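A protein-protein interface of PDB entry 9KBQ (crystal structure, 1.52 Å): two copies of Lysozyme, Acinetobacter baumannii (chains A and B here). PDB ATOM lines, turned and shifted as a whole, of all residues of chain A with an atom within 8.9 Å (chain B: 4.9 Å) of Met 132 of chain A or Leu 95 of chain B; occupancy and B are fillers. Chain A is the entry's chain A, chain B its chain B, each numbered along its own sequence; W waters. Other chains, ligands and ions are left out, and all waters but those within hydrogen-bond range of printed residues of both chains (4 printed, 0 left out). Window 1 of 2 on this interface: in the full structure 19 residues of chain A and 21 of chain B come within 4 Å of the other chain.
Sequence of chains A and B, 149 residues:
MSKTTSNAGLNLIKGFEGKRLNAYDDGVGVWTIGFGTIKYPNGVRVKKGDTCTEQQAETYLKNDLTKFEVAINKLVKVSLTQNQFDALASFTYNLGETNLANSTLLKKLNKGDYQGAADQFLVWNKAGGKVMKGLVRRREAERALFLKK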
ATOM      1  N   ASP A  26       0.132   0.252  37.920  1.00  0.00           N
ATOM      2  CA  ASP A  26       0.373  -0.383  36.629  1.00  0.00           C
ATOM      3  C   ASP A  26      -0.634  -1.480  36.304  1.00  0.00           C
ATOM      4  O   ASP A  26      -0.548  -2.078  35.223  1.00  0.00           O
ATOM      5  CB  ASP A  26       1.804  -0.937  36.562  1.00  0.00           C
ATOM      6  CG  ASP A  26       2.031  -2.114  37.488  1.00  0.00           C
ATOM      7  OD1 ASP A  26       1.129  -2.455  38.284  1.00  0.00           O
ATOM      8  OD2 ASP A  26       3.127  -2.713  37.411  1.00  0.00           O
ATOM      9  N   GLY A  27      -1.579  -1.761  37.201  1.00  0.00           N
ATOM     10  CA  GLY A  27      -2.605  -2.756  36.957  1.00  0.00           C
ATOM     11  C   GLY A  27      -2.389  -4.061  37.689  1.00  0.00           C
ATOM     12  O   GLY A  27      -3.333  -4.862  37.798  1.00  0.00           O
ATOM     13  N   ASN A  94      13.580  -4.802  29.724  1.00  0.00           N
ATOM     14  CA  ASN A  94      12.207  -5.189  29.416  1.00  0.00           C
ATOM     15  C   ASN A  94      11.934  -6.659  29.728  1.00  0.00           C
ATOM     16  O   ASN A  94      10.865  -6.997  30.256  1.00  0.00           O
ATOM     17  CB  ASN A  94      11.934  -4.874  27.943  1.00  0.00           C
ATOM     18  CG  ASN A  94      10.507  -5.114  27.541  1.00  0.00           C
ATOM     19  OD1 ASN A  94      10.245  -5.568  26.432  1.00  0.00           O
ATOM     20  ND2 ASN A  94       9.572  -4.823  28.441  1.00  0.00           N
ATOM     21  N   LEU A 122      14.301  -9.950  17.384  1.00  0.00           N
ATOM     22  CA  LEU A 122      12.956  -9.832  16.837  1.00  0.00           C
ATOM     23  C   LEU A 122      12.014 -10.937  17.287  1.00  0.00           C
ATOM     24  O   LEU A 122      10.798 -10.803  17.100  1.00  0.00           O
ATOM     25  CB  LEU A 122      13.023  -9.823  15.307  1.00  0.00           C
ATOM     26  CG  LEU A 122      13.862  -8.707  14.682  1.00  0.00           C
ATOM     27  CD1 LEU A 122      13.881  -8.874  13.168  1.00  0.00           C
ATOM     28  CD2 LEU A 122      13.304  -7.352  15.085  1.00  0.00           C
ATOM     29  N   TRP A 124      11.362 -11.828  20.304  1.00  0.00           N
ATOM     30  CA  TRP A 124      10.811 -11.533  21.630  1.00  0.00           C
ATOM     31  C   TRP A 124       9.727 -10.458  21.539  1.00  0.00           C
ATOM     32  O   TRP A 124       9.823  -9.378  22.121  1.00  0.00           O
ATOM     33  CB  TRP A 124      11.928 -11.103  22.575  1.00  0.00           C
ATOM     34  CG  TRP A 124      12.892 -12.191  22.842  1.00  0.00           C
ATOM     35  CD1 TRP A 124      13.973 -12.537  22.074  1.00  0.00           C
ATOM     36  CD2 TRP A 124      12.860 -13.113  23.926  1.00  0.00           C
ATOM     37  NE1 TRP A 124      14.623 -13.609  22.630  1.00  0.00           N
ATOM     38  CE2 TRP A 124      13.954 -13.984  23.771  1.00  0.00           C
ATOM     39  CE3 TRP A 124      12.010 -13.287  25.027  1.00  0.00           C
ATOM     40  CZ2 TRP A 124      14.225 -15.012  24.668  1.00  0.00           C
ATOM     41  CZ3 TRP A 124      12.284 -14.300  25.921  1.00  0.00           C
ATOM     42  CH2 TRP A 124      13.382 -15.152  25.738  1.00  0.00           C
ATOM     43  N   ASN A 125       8.662 -10.781  20.802  1.00  0.00           N
ATOM     44  CA  ASN A 125       7.610  -9.813  20.526  1.00  0.00           C
ATOM     45  C   ASN A 125       6.269 -10.213  21.140  1.00  0.00           C
ATOM     46  O   ASN A 125       5.239  -9.654  20.762  1.00  0.00           O
ATOM     47  CB  ASN A 125       7.459  -9.604  19.019  1.00  0.00           C
ATOM     48  CG  ASN A 125       7.129 -10.885  18.276  1.00  0.00           C
ATOM     49  OD1 ASN A 125       6.791 -11.911  18.878  1.00  0.00           O
ATOM     50  ND2 ASN A 125       7.229 -10.835  16.951  1.00  0.00           N
ATOM     51  N   LYS A 126       6.266 -11.156  22.079  1.00  0.00           N
ATOM     52  CA  LYS A 126       5.044 -11.715  22.643  1.00  0.00           C
ATOM     53  C   LYS A 126       4.919 -11.386  24.128  1.00  0.00           C
ATOM     54  O   LYS A 126       5.914 -11.253  24.846  1.00  0.00           O
ATOM     55  CB  LYS A 126       5.011 -13.237  22.452  1.00  0.00           C
ATOM     56  CG  LYS A 126       4.484 -13.682  21.097  1.00  0.00           C
ATOM     57  CD  LYS A 126       4.774 -15.158  20.836  1.00  0.00           C
ATOM     58  CE  LYS A 126       5.070 -15.434  19.365  1.00  0.00           C
ATOM     59  NZ  LYS A 126       6.142 -14.562  18.811  1.00  0.00           N
ATOM     60  N   ALA A 127       3.675 -11.257  24.584  1.00  0.00           N
ATOM     61  CA  ALA A 127       3.375 -11.104  26.001  1.00  0.00           C
ATOM     62  C   ALA A 127       2.073 -11.836  26.263  1.00  0.00           C
ATOM     63  O   ALA A 127       1.070 -11.560  25.596  1.00  0.00           O
ATOM     64  CB  ALA A 127       3.256  -9.633  26.407  1.00  0.00           C
ATOM     65  N   GLY A 128       2.097 -12.777  27.203  1.00  0.00           N
ATOM     66  CA  GLY A 128       0.897 -13.531  27.538  1.00  0.00           C
ATOM     67  C   GLY A 128       0.264 -14.237  26.361  1.00  0.00           C
ATOM     68  O   GLY A 128      -0.967 -14.283  26.261  1.00  0.00           O
ATOM     69  N   GLY A 129       1.076 -14.786  25.456  1.00  0.00           N
ATOM     70  CA  GLY A 129       0.572 -15.476  24.287  1.00  0.00           C
ATOM     71  C   GLY A 129       0.155 -14.588  23.134  1.00  0.00           C
ATOM     72  O   GLY A 129      -0.377 -15.102  22.141  1.00  0.00           O
ATOM     73  N   LYS A 130       0.384 -13.281  23.227  1.00  0.00           N
ATOM     74  CA  LYS A 130      -0.146 -12.302  22.286  1.00  0.00           C
ATOM     75  C   LYS A 130       1.021 -11.545  21.663  1.00  0.00           C
ATOM     76  O   LYS A 130       1.798 -10.906  22.379  1.00  0.00           O
ATOM     77  CB  LYS A 130      -1.100 -11.338  23.006  1.00  0.00           C
ATOM     78  CG  LYS A 130      -1.756 -10.270  22.138  1.00  0.00           C
ATOM     79  CD  LYS A 130      -2.800 -10.881  21.211  1.00  0.00           C
ATOM     80  CE  LYS A 130      -3.227  -9.914  20.124  1.00  0.00           C
ATOM     81  NZ  LYS A 130      -4.287  -8.984  20.601  1.00  0.00           N
ATOM     82  N   VAL A 131       1.142 -11.614  20.338  1.00  0.00           N
ATOM     83  CA  VAL A 131       2.105 -10.758  19.651  1.00  0.00           C
ATOM     84  C   VAL A 131       1.666  -9.311  19.810  1.00  0.00           C
ATOM     85  O   VAL A 131       0.530  -8.948  19.471  1.00  0.00           O
ATOM     86  CB  VAL A 131       2.232 -11.144  18.172  1.00  0.00           C
ATOM     87  CG1 VAL A 131       3.066 -10.106  17.434  1.00  0.00           C
ATOM     88  CG2 VAL A 131       2.874 -12.514  18.038  1.00  0.00           C
ATOM     89  N   MET A 132       2.557  -8.481  20.346  1.00  0.00           N
ATOM     90  CA  MET A 132       2.259  -7.095  20.677  1.00  0.00           C
ATOM     91  C   MET A 132       2.977  -6.176  19.698  1.00  0.00           C
ATOM     92  O   MET A 132       4.191  -6.296  19.514  1.00  0.00           O
ATOM     93  CB  MET A 132       2.696  -6.779  22.110  1.00  0.00           C
ATOM     94  CG  MET A 132       2.065  -7.669  23.163  1.00  0.00           C
ATOM     95  SD  MET A 132       0.518  -6.992  23.778  1.00  0.00           S
ATOM     96  CE  MET A 132       0.092  -8.208  25.026  1.00  0.00           C
ATOM     97  N   LYS A 133       2.227  -5.261  19.077  1.00  0.00           N
ATOM     98  CA  LYS A 133       2.838  -4.294  18.166  1.00  0.00           C
ATOM     99  C   LYS A 133       3.918  -3.478  18.866  1.00  0.00           C
ATOM    100  O   LYS A 133       4.993  -3.242  18.298  1.00  0.00           O
ATOM    101  CB  LYS A 133       1.771  -3.366  17.587  1.00  0.00           C
ATOM    102  CG  LYS A 133       0.979  -3.948  16.430  1.00  0.00           C
ATOM    103  CD  LYS A 133       0.104  -2.873  15.791  1.00  0.00           C
ATOM    104  CE  LYS A 133      -1.362  -3.055  16.152  1.00  0.00           C
ATOM    105  NZ  LYS A 133      -2.254  -2.422  15.138  1.00  0.00           N
ATOM    106  N   GLY A 134       3.647  -3.035  20.096  1.00  0.00           N
ATOM    107  CA  GLY A 134       4.633  -2.255  20.827  1.00  0.00           C
ATOM    108  C   GLY A 134       5.919  -3.018  21.073  1.00  0.00           C
ATOM    109  O   GLY A 134       7.014  -2.450  21.005  1.00  0.00           O
ATOM    110  N   LEU A 135       5.810  -4.319  21.351  1.00  0.00           N
ATOM    111  CA  LEU A 135       7.010  -5.120  21.556  1.00  0.00           C
ATOM    112  C   LEU A 135       7.776  -5.298  20.253  1.00  0.00           C
ATOM    113  O   LEU A 135       9.010  -5.267  20.254  1.00  0.00           O
ATOM    114  CB  LEU A 135       6.654  -6.480  22.156  1.00  0.00           C
ATOM    115  CG  LEU A 135       6.045  -6.469  23.559  1.00  0.00           C
ATOM    116  CD1 LEU A 135       5.835  -7.895  24.052  1.00  0.00           C
ATOM    117  CD2 LEU A 135       6.927  -5.679  24.521  1.00  0.00           C
ATOM    118  N   VAL A 136       7.068  -5.490  19.134  1.00  0.00           N
ATOM    119  CA  VAL A 136       7.748  -5.543  17.839  1.00  0.00           C
ATOM    120  C   VAL A 136       8.517  -4.251  17.604  1.00  0.00           C
ATOM    121  O   VAL A 136       9.670  -4.264  17.149  1.00  0.00           O
ATOM    122  CB  VAL A 136       6.747  -5.808  16.698  1.00  0.00           C
ATOM    123  CG1 VAL A 136       7.477  -5.824  15.353  1.00  0.00           C
ATOM    124  CG2 VAL A 136       6.018  -7.114  16.912  1.00  0.00           C
ATOM    125  N   ARG A 137       7.892  -3.113  17.916  1.00  0.00           N
ATOM    126  CA  ARG A 137       8.556  -1.823  17.745  1.00  0.00           C
ATOM    127  C   ARG A 137       9.812  -1.728  18.604  1.00  0.00           C
ATOM    128  O   ARG A 137      10.877  -1.298  18.131  1.00  0.00           O
ATOM    129  CB  ARG A 137       7.585  -0.691  18.080  1.00  0.00           C
ATOM    130  CG  ARG A 137       7.174   0.127  16.872  1.00  0.00           C
ATOM    131  CD  ARG A 137       6.024   1.062  17.191  1.00  0.00           C
ATOM    132  NE  ARG A 137       5.109   1.144  16.061  1.00  0.00           N
ATOM    133  CZ  ARG A 137       3.826   0.820  16.108  1.00  0.00           C
ATOM    134  NH1 ARG A 137       3.257   0.402  17.226  1.00  0.00           N
ATOM    135  NH2 ARG A 137       3.098   0.904  14.999  1.00  0.00           N
ATOM    136  N   ARG A 138       9.708  -2.120  19.875  1.00  0.00           N
ATOM    137  CA  ARG A 138      10.871  -2.101  20.757  1.00  0.00           C
ATOM    138  C   ARG A 138      11.993  -2.973  20.213  1.00  0.00           C
ATOM    139  O   ARG A 138      13.159  -2.558  20.177  1.00  0.00           O
ATOM    140  CB  ARG A 138      10.486  -2.560  22.163  1.00  0.00           C
ATOM    141  CG  ARG A 138       9.497  -1.673  22.875  1.00  0.00           C
ATOM    142  CD  ARG A 138       9.136  -2.275  24.221  1.00  0.00           C
ATOM    143  NE  ARG A 138       7.797  -1.897  24.654  1.00  0.00           N
ATOM    144  CZ  ARG A 138       7.248  -2.281  25.797  1.00  0.00           C
ATOM    145  NH1 ARG A 138       7.878  -3.101  26.623  1.00  0.00           N
ATOM    146  NH2 ARG A 138       6.037  -1.838  26.117  1.00  0.00           N
ATOM    147  N   ARG A 139      11.652  -4.191  19.777  1.00  0.00           N
ATOM    148  CA  ARG A 139      12.672  -5.126  19.315  1.00  0.00           C
ATOM    149  C   ARG A 139      13.327  -4.632  18.032  1.00  0.00           C
ATOM    150  O   ARG A 139      14.541  -4.778  17.858  1.00  0.00           O
ATOM    151  CB  ARG A 139      12.068  -6.513  19.102  1.00  0.00           C
ATOM    152  CG  ARG A 139      11.466  -7.146  20.367  1.00  0.00           C
ATOM    153  CD  ARG A 139      12.503  -7.446  21.444  1.00  0.00           C
ATOM    154  NE  ARG A 139      12.692  -6.358  22.398  1.00  0.00           N
ATOM    155  CZ  ARG A 139      11.941  -6.158  23.475  1.00  0.00           C
ATOM    156  NH1 ARG A 139      10.881  -6.910  23.734  1.00  0.00           N
ATOM    157  NH2 ARG A 139      12.266  -5.181  24.317  1.00  0.00           N
ATOM    158  N   GLU A 140      12.544  -4.044  17.126  1.00  0.00           N
ATOM    159  CA  GLU A 140      13.126  -3.531  15.889  1.00  0.00           C
ATOM    160  C   GLU A 140      14.042  -2.345  16.166  1.00  0.00           C
ATOM    161  O   GLU A 140      15.107  -2.221  15.547  1.00  0.00           O
ATOM    162  CB  GLU A 140      12.020  -3.167  14.897  1.00  0.00           C
ATOM    163  CG  GLU A 140      11.210  -4.392  14.436  1.00  0.00           C
ATOM    164  CD  GLU A 140      10.124  -4.065  13.420  1.00  0.00           C
ATOM    165  OE1 GLU A 140       9.493  -2.994  13.543  1.00  0.00           O
ATOM    166  OE2 GLU A 140       9.880  -4.891  12.513  1.00  0.00           O
ATOM    167  N   PHE B  91     -10.703  -7.941  27.083  1.00  0.00           N
ATOM    168  CA  PHE B  91      -9.567  -7.469  27.876  1.00  0.00           C
ATOM    169  C   PHE B  91      -8.341  -8.358  27.672  1.00  0.00           C
ATOM    170  O   PHE B  91      -7.224  -7.866  27.445  1.00  0.00           O
ATOM    171  CB  PHE B  91     -10.010  -7.438  29.344  1.00  0.00           C
ATOM    172  CG  PHE B  91      -8.947  -7.023  30.324  1.00  0.00           C
ATOM    173  CD1 PHE B  91      -8.107  -7.965  30.902  1.00  0.00           C
ATOM    174  CD2 PHE B  91      -8.848  -5.702  30.729  1.00  0.00           C
ATOM    175  CE1 PHE B  91      -7.143  -7.578  31.833  1.00  0.00           C
ATOM    176  CE2 PHE B  91      -7.898  -5.310  31.663  1.00  0.00           C
ATOM    177  CZ  PHE B  91      -7.046  -6.253  32.211  1.00  0.00           C
ATOM    178  N   THR B  92      -8.534  -9.675  27.734  1.00  0.00           N
ATOM    179  CA  THR B  92      -7.430 -10.623  27.693  1.00  0.00           C
ATOM    180  C   THR B  92      -6.884 -10.783  26.282  1.00  0.00           C
ATOM    181  O   THR B  92      -5.671 -10.950  26.110  1.00  0.00           O
ATOM    182  CB  THR B  92      -7.899 -11.970  28.247  1.00  0.00           C
ATOM    183  OG1 THR B  92      -8.435 -11.778  29.567  1.00  0.00           O
ATOM    184  CG2 THR B  92      -6.747 -12.956  28.326  1.00  0.00           C
ATOM    185  N   TYR B  93      -7.756 -10.726  25.271  1.00  0.00           N
ATOM    186  CA  TYR B  93      -7.300 -10.694  23.885  1.00  0.00           C
ATOM    187  C   TYR B  93      -6.421  -9.484  23.630  1.00  0.00           C
ATOM    188  O   TYR B  93      -5.458  -9.563  22.855  1.00  0.00           O
ATOM    189  CB  TYR B  93      -8.511 -10.679  22.950  1.00  0.00           C
ATOM    190  CG  TYR B  93      -8.182 -10.567  21.480  1.00  0.00           C
ATOM    191  CD1 TYR B  93      -7.863 -11.691  20.735  1.00  0.00           C
ATOM    192  CD2 TYR B  93      -8.198  -9.337  20.840  1.00  0.00           C
ATOM    193  CE1 TYR B  93      -7.560 -11.589  19.386  1.00  0.00           C
ATOM    194  CE2 TYR B  93      -7.894  -9.223  19.498  1.00  0.00           C
ATOM    195  CZ  TYR B  93      -7.581 -10.354  18.776  1.00  0.00           C
ATOM    196  OH  TYR B  93      -7.277 -10.245  17.437  1.00  0.00           O
ATOM    197  N   ASN B  94      -6.732  -8.358  24.279  1.00  0.00           N
ATOM    198  CA  ASN B  94      -5.936  -7.153  24.072  1.00  0.00           C
ATOM    199  C   ASN B  94      -4.624  -7.192  24.856  1.00  0.00           C
ATOM    200  O   ASN B  94      -3.569  -6.824  24.319  1.00  0.00           O
ATOM    201  CB  ASN B  94      -6.772  -5.932  24.454  1.00  0.00           C
ATOM    202  CG  ASN B  94      -6.045  -4.628  24.230  1.00  0.00           C
ATOM    203  OD1 ASN B  94      -6.040  -3.752  25.096  1.00  0.00           O
ATOM    204  ND2 ASN B  94      -5.430  -4.484  23.064  1.00  0.00           N
ATOM    205  N   LEU B  95      -4.658  -7.646  26.114  1.00  0.00           N
ATOM    206  CA  LEU B  95      -3.522  -7.498  27.019  1.00  0.00           C
ATOM    207  C   LEU B  95      -2.744  -8.783  27.276  1.00  0.00           C
ATOM    208  O   LEU B  95      -1.661  -8.718  27.867  1.00  0.00           O
ATOM    209  CB  LEU B  95      -3.997  -6.914  28.361  1.00  0.00           C
ATOM    210  CG  LEU B  95      -4.515  -5.482  28.270  1.00  0.00           C
ATOM    211  CD1 LEU B  95      -5.334  -5.132  29.494  1.00  0.00           C
ATOM    212  CD2 LEU B  95      -3.358  -4.505  28.143  1.00  0.00           C
ATOM    213  N   GLY B  96      -3.243  -9.935  26.848  1.00  0.00           N
ATOM    214  CA  GLY B  96      -2.542 -11.184  27.057  1.00  0.00           C
ATOM    215  C   GLY B  96      -2.901 -11.857  28.373  1.00  0.00           C
ATOM    216  O   GLY B  96      -3.406 -11.241  29.313  1.00  0.00           O
ATOM    217  N   GLU B  97      -2.595 -13.156  28.438  1.00  0.00           N
ATOM    218  CA  GLU B  97      -2.975 -13.967  29.593  1.00  0.00           C
ATOM    219  C   GLU B  97      -2.154 -13.649  30.834  1.00  0.00           C
ATOM    220  O   GLU B  97      -2.658 -13.790  31.950  1.00  0.00           O
ATOM    221  CB  GLU B  97      -2.846 -15.458  29.275  1.00  0.00           C
ATOM    222  CG  GLU B  97      -3.120 -15.826  27.837  1.00  0.00           C
ATOM    223  CD  GLU B  97      -2.870 -17.292  27.565  1.00  0.00           C
ATOM    224  OE1 GLU B  97      -2.682 -18.055  28.539  1.00  0.00           O
ATOM    225  OE2 GLU B  97      -2.850 -17.680  26.378  1.00  0.00           O
ATOM    226  N   ASN B  99      -0.960 -10.658  31.820  1.00  0.00           N
ATOM    227  CA  ASN B  99      -1.523  -9.467  32.441  1.00  0.00           C
ATOM    228  C   ASN B  99      -2.814  -9.787  33.188  1.00  0.00           C
ATOM    229  O   ASN B  99      -3.030  -9.280  34.294  1.00  0.00           O
ATOM    230  CB  ASN B  99      -1.746  -8.377  31.394  1.00  0.00           C
ATOM    231  CG  ASN B  99      -0.477  -7.590  31.101  1.00  0.00           C
ATOM    232  OD1 ASN B  99       0.351  -7.367  31.992  1.00  0.00           O
ATOM    233  ND2 ASN B  99      -0.317  -7.169  29.850  1.00  0.00           N
ATOM    234  N   TRP B 124      -6.118  -0.108  33.136  1.00  0.00           N
ATOM    235  CA  TRP B 124      -5.300  -0.583  32.020  1.00  0.00           C
ATOM    236  C   TRP B 124      -5.512   0.291  30.783  1.00  0.00           C
ATOM    237  O   TRP B 124      -5.938  -0.169  29.720  1.00  0.00           O
ATOM    238  CB  TRP B 124      -5.625  -2.042  31.716  1.00  0.00           C
ATOM    239  CG  TRP B 124      -5.250  -2.998  32.800  1.00  0.00           C
ATOM    240  CD1 TRP B 124      -5.981  -3.305  33.917  1.00  0.00           C
ATOM    241  CD2 TRP B 124      -4.046  -3.761  32.886  1.00  0.00           C
ATOM    242  NE1 TRP B 124      -5.312  -4.232  34.677  1.00  0.00           N
ATOM    243  CE2 TRP B 124      -4.113  -4.517  34.071  1.00  0.00           C
ATOM    244  CE3 TRP B 124      -2.908  -3.876  32.074  1.00  0.00           C
ATOM    245  CZ2 TRP B 124      -3.103  -5.395  34.453  1.00  0.00           C
ATOM    246  CZ3 TRP B 124      -1.903  -4.737  32.459  1.00  0.00           C
ATOM    247  CH2 TRP B 124      -2.000  -5.478  33.643  1.00  0.00           C
ATOM    248  N   ARG B 139     -11.481   0.261  27.585  1.00  0.00           N
ATOM    249  CA  ARG B 139     -11.671  -0.223  28.948  1.00  0.00           C
ATOM    250  C   ARG B 139     -13.031   0.183  29.494  1.00  0.00           C
ATOM    251  O   ARG B 139     -13.642  -0.565  30.266  1.00  0.00           O
ATOM    252  CB  ARG B 139     -10.556   0.295  29.856  1.00  0.00           C
ATOM    253  CG  ARG B 139      -9.173  -0.197  29.478  1.00  0.00           C
ATOM    254  CD  ARG B 139      -9.010  -1.702  29.699  1.00  0.00           C
ATOM    255  NE  ARG B 139      -9.232  -2.516  28.507  1.00  0.00           N
ATOM    256  CZ  ARG B 139      -8.307  -2.771  27.589  1.00  0.00           C
ATOM    257  NH1 ARG B 139      -7.098  -2.233  27.653  1.00  0.00           N
ATOM    258  NH2 ARG B 139      -8.600  -3.590  26.583  1.00  0.00           N
HETATM  259  O   HOH W   1      -5.421  -6.152  20.502  1.00  0.00           O
HETATM  260  O   HOH W   2      -2.790  -6.552  21.483  1.00  0.00           O
HETATM  261  O   HOH W   3      -5.981  -4.630  37.478  1.00  0.00           O
HETATM  262  O   HOH W   4      -1.790  -4.491  24.501  1.00  0.00           O
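O of Gly 128 of chain A sits at hydrogen-bond distance from N of Glu 97 of chain B (2.9 Å).
O of Tyr 93 of chain B lies within hydrogen-bond range of NZ of Lys 130 of chain A.
N of Met 132 of chain A sits at hydrogen-bond distance from O of Asn 125 of chain A (3.0 Å).
OD1 of Asn 94 of chain B lies within hydrogen-bond range of NH2 of Arg 139 of chain B (3.0 Å).
The side-chain amide nitrogen (ND2) of Asn 99 of chain B sits at hydrogen-bond distance from the backbone carbonyl oxygen (O) of Leu 95 of chain B (2.9 Å).
The backbone carbonyl oxygen (O) of Trp 124 of chain B lies within hydrogen-bond range of the guanidinium group (NH1) of Arg 139 of chain B, 3.1 Å away.
Among the printed residues, pairs that only touch across the chains: Gly 27 of chain A with Trp 124 of chain B, Ala 127 of chain A with Gly 96 of chain B, Gly 128 of chain A with Gly 96 of chain B, Met 132 of chain A with Asn 94 of chain B and Met 132 of chain A with Leu 95 of chain B.
Met 132 of chain A touches just these residues of chain B: Asn 94 (3.98 Å) and Leu 95 (3.4 Å).
Of chain A, only Met 132 (3.4 Å) comes within 4 Å of Leu 95 of chain B.
Asn 94 of chain B touches just one residue of chain A: Met 132 (3.98 Å).
Gly 96 of chain B touches just these residues of chain A: Ala 127 and Gly 128.
Of the printed residues of chain A, Trp 124 of chain B touches Gly 27 (3.4 Å).
Printed residues of chain A within 4 Å of Glu 97 of chain B: Gly 128.
Printed residues of chain B within 4 Å of Gly 128 of chain A: Gly 96 (3.6 Å) and Glu 97 (2.9 Å).
Printed residues of chain B within 4 Å of Gly 27 of chain A: Trp 124 (3.4 Å).
Lys 133 of chain A touches none of the printed residues of chain B.
Gly 134 of chain A touches none of the printed residues of chain B.
The nearest residue of chain B that does not touch Met 132 of chain A is Gly 96 of chain B (4.2 Å).
The nearest printed residue of chain A that does not touch Trp 124 of chain B is Asp 26 of chain A (4.02 Å).
Of the 21 printed residues of chain A, 5 touch a printed residue of chain B.
Printed residues of chain A that touch a printed residue of chain B: Gly 27, Ala 127, Gly 128, Lys 130 and Met 132.
Of the 10 printed residues of chain B, 6 touch a printed residue of chain A.
Hydrophobic or aromatic side chains of chain B within 4 Å of the printed part of chain A: Tyr 93 and Trp 124.
Among the printed residues, no Asp or Glu carboxylate lies within 4 Å of a Lys or Arg side-chain nitrogen of the other chain.
3 positions are printed for both chains.
Of the 7 pairs that touch across the chains among the printed residues, none has its exchanged pair printed and touching as well.
Water W3 lies within hydrogen-bond range of the backbone carbonyl oxygen of Gly 27 of chain A (2.7 Å) and the indole nitrogen of Trp 124 of chain B (2.9 Å).
Water W4 bridges the backbone carbonyl oxygen (O) of Asn 94 of chain B and the side-chain sulfur (SD) of Met 132 of chain A.
Water W2 lies within hydrogen-bond range of the backbone carbonyl oxygen (O) of Asn 94 of chain B and the side-chain amino group (NZ) of Lys 130 of chain A.
Water W1 bridges the side-chain amino group (NZ) of Lys 130 of chain A (3.1 Å) and the side-chain amide nitrogen (ND2) of Asn 94 of chain B (3.1 Å).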
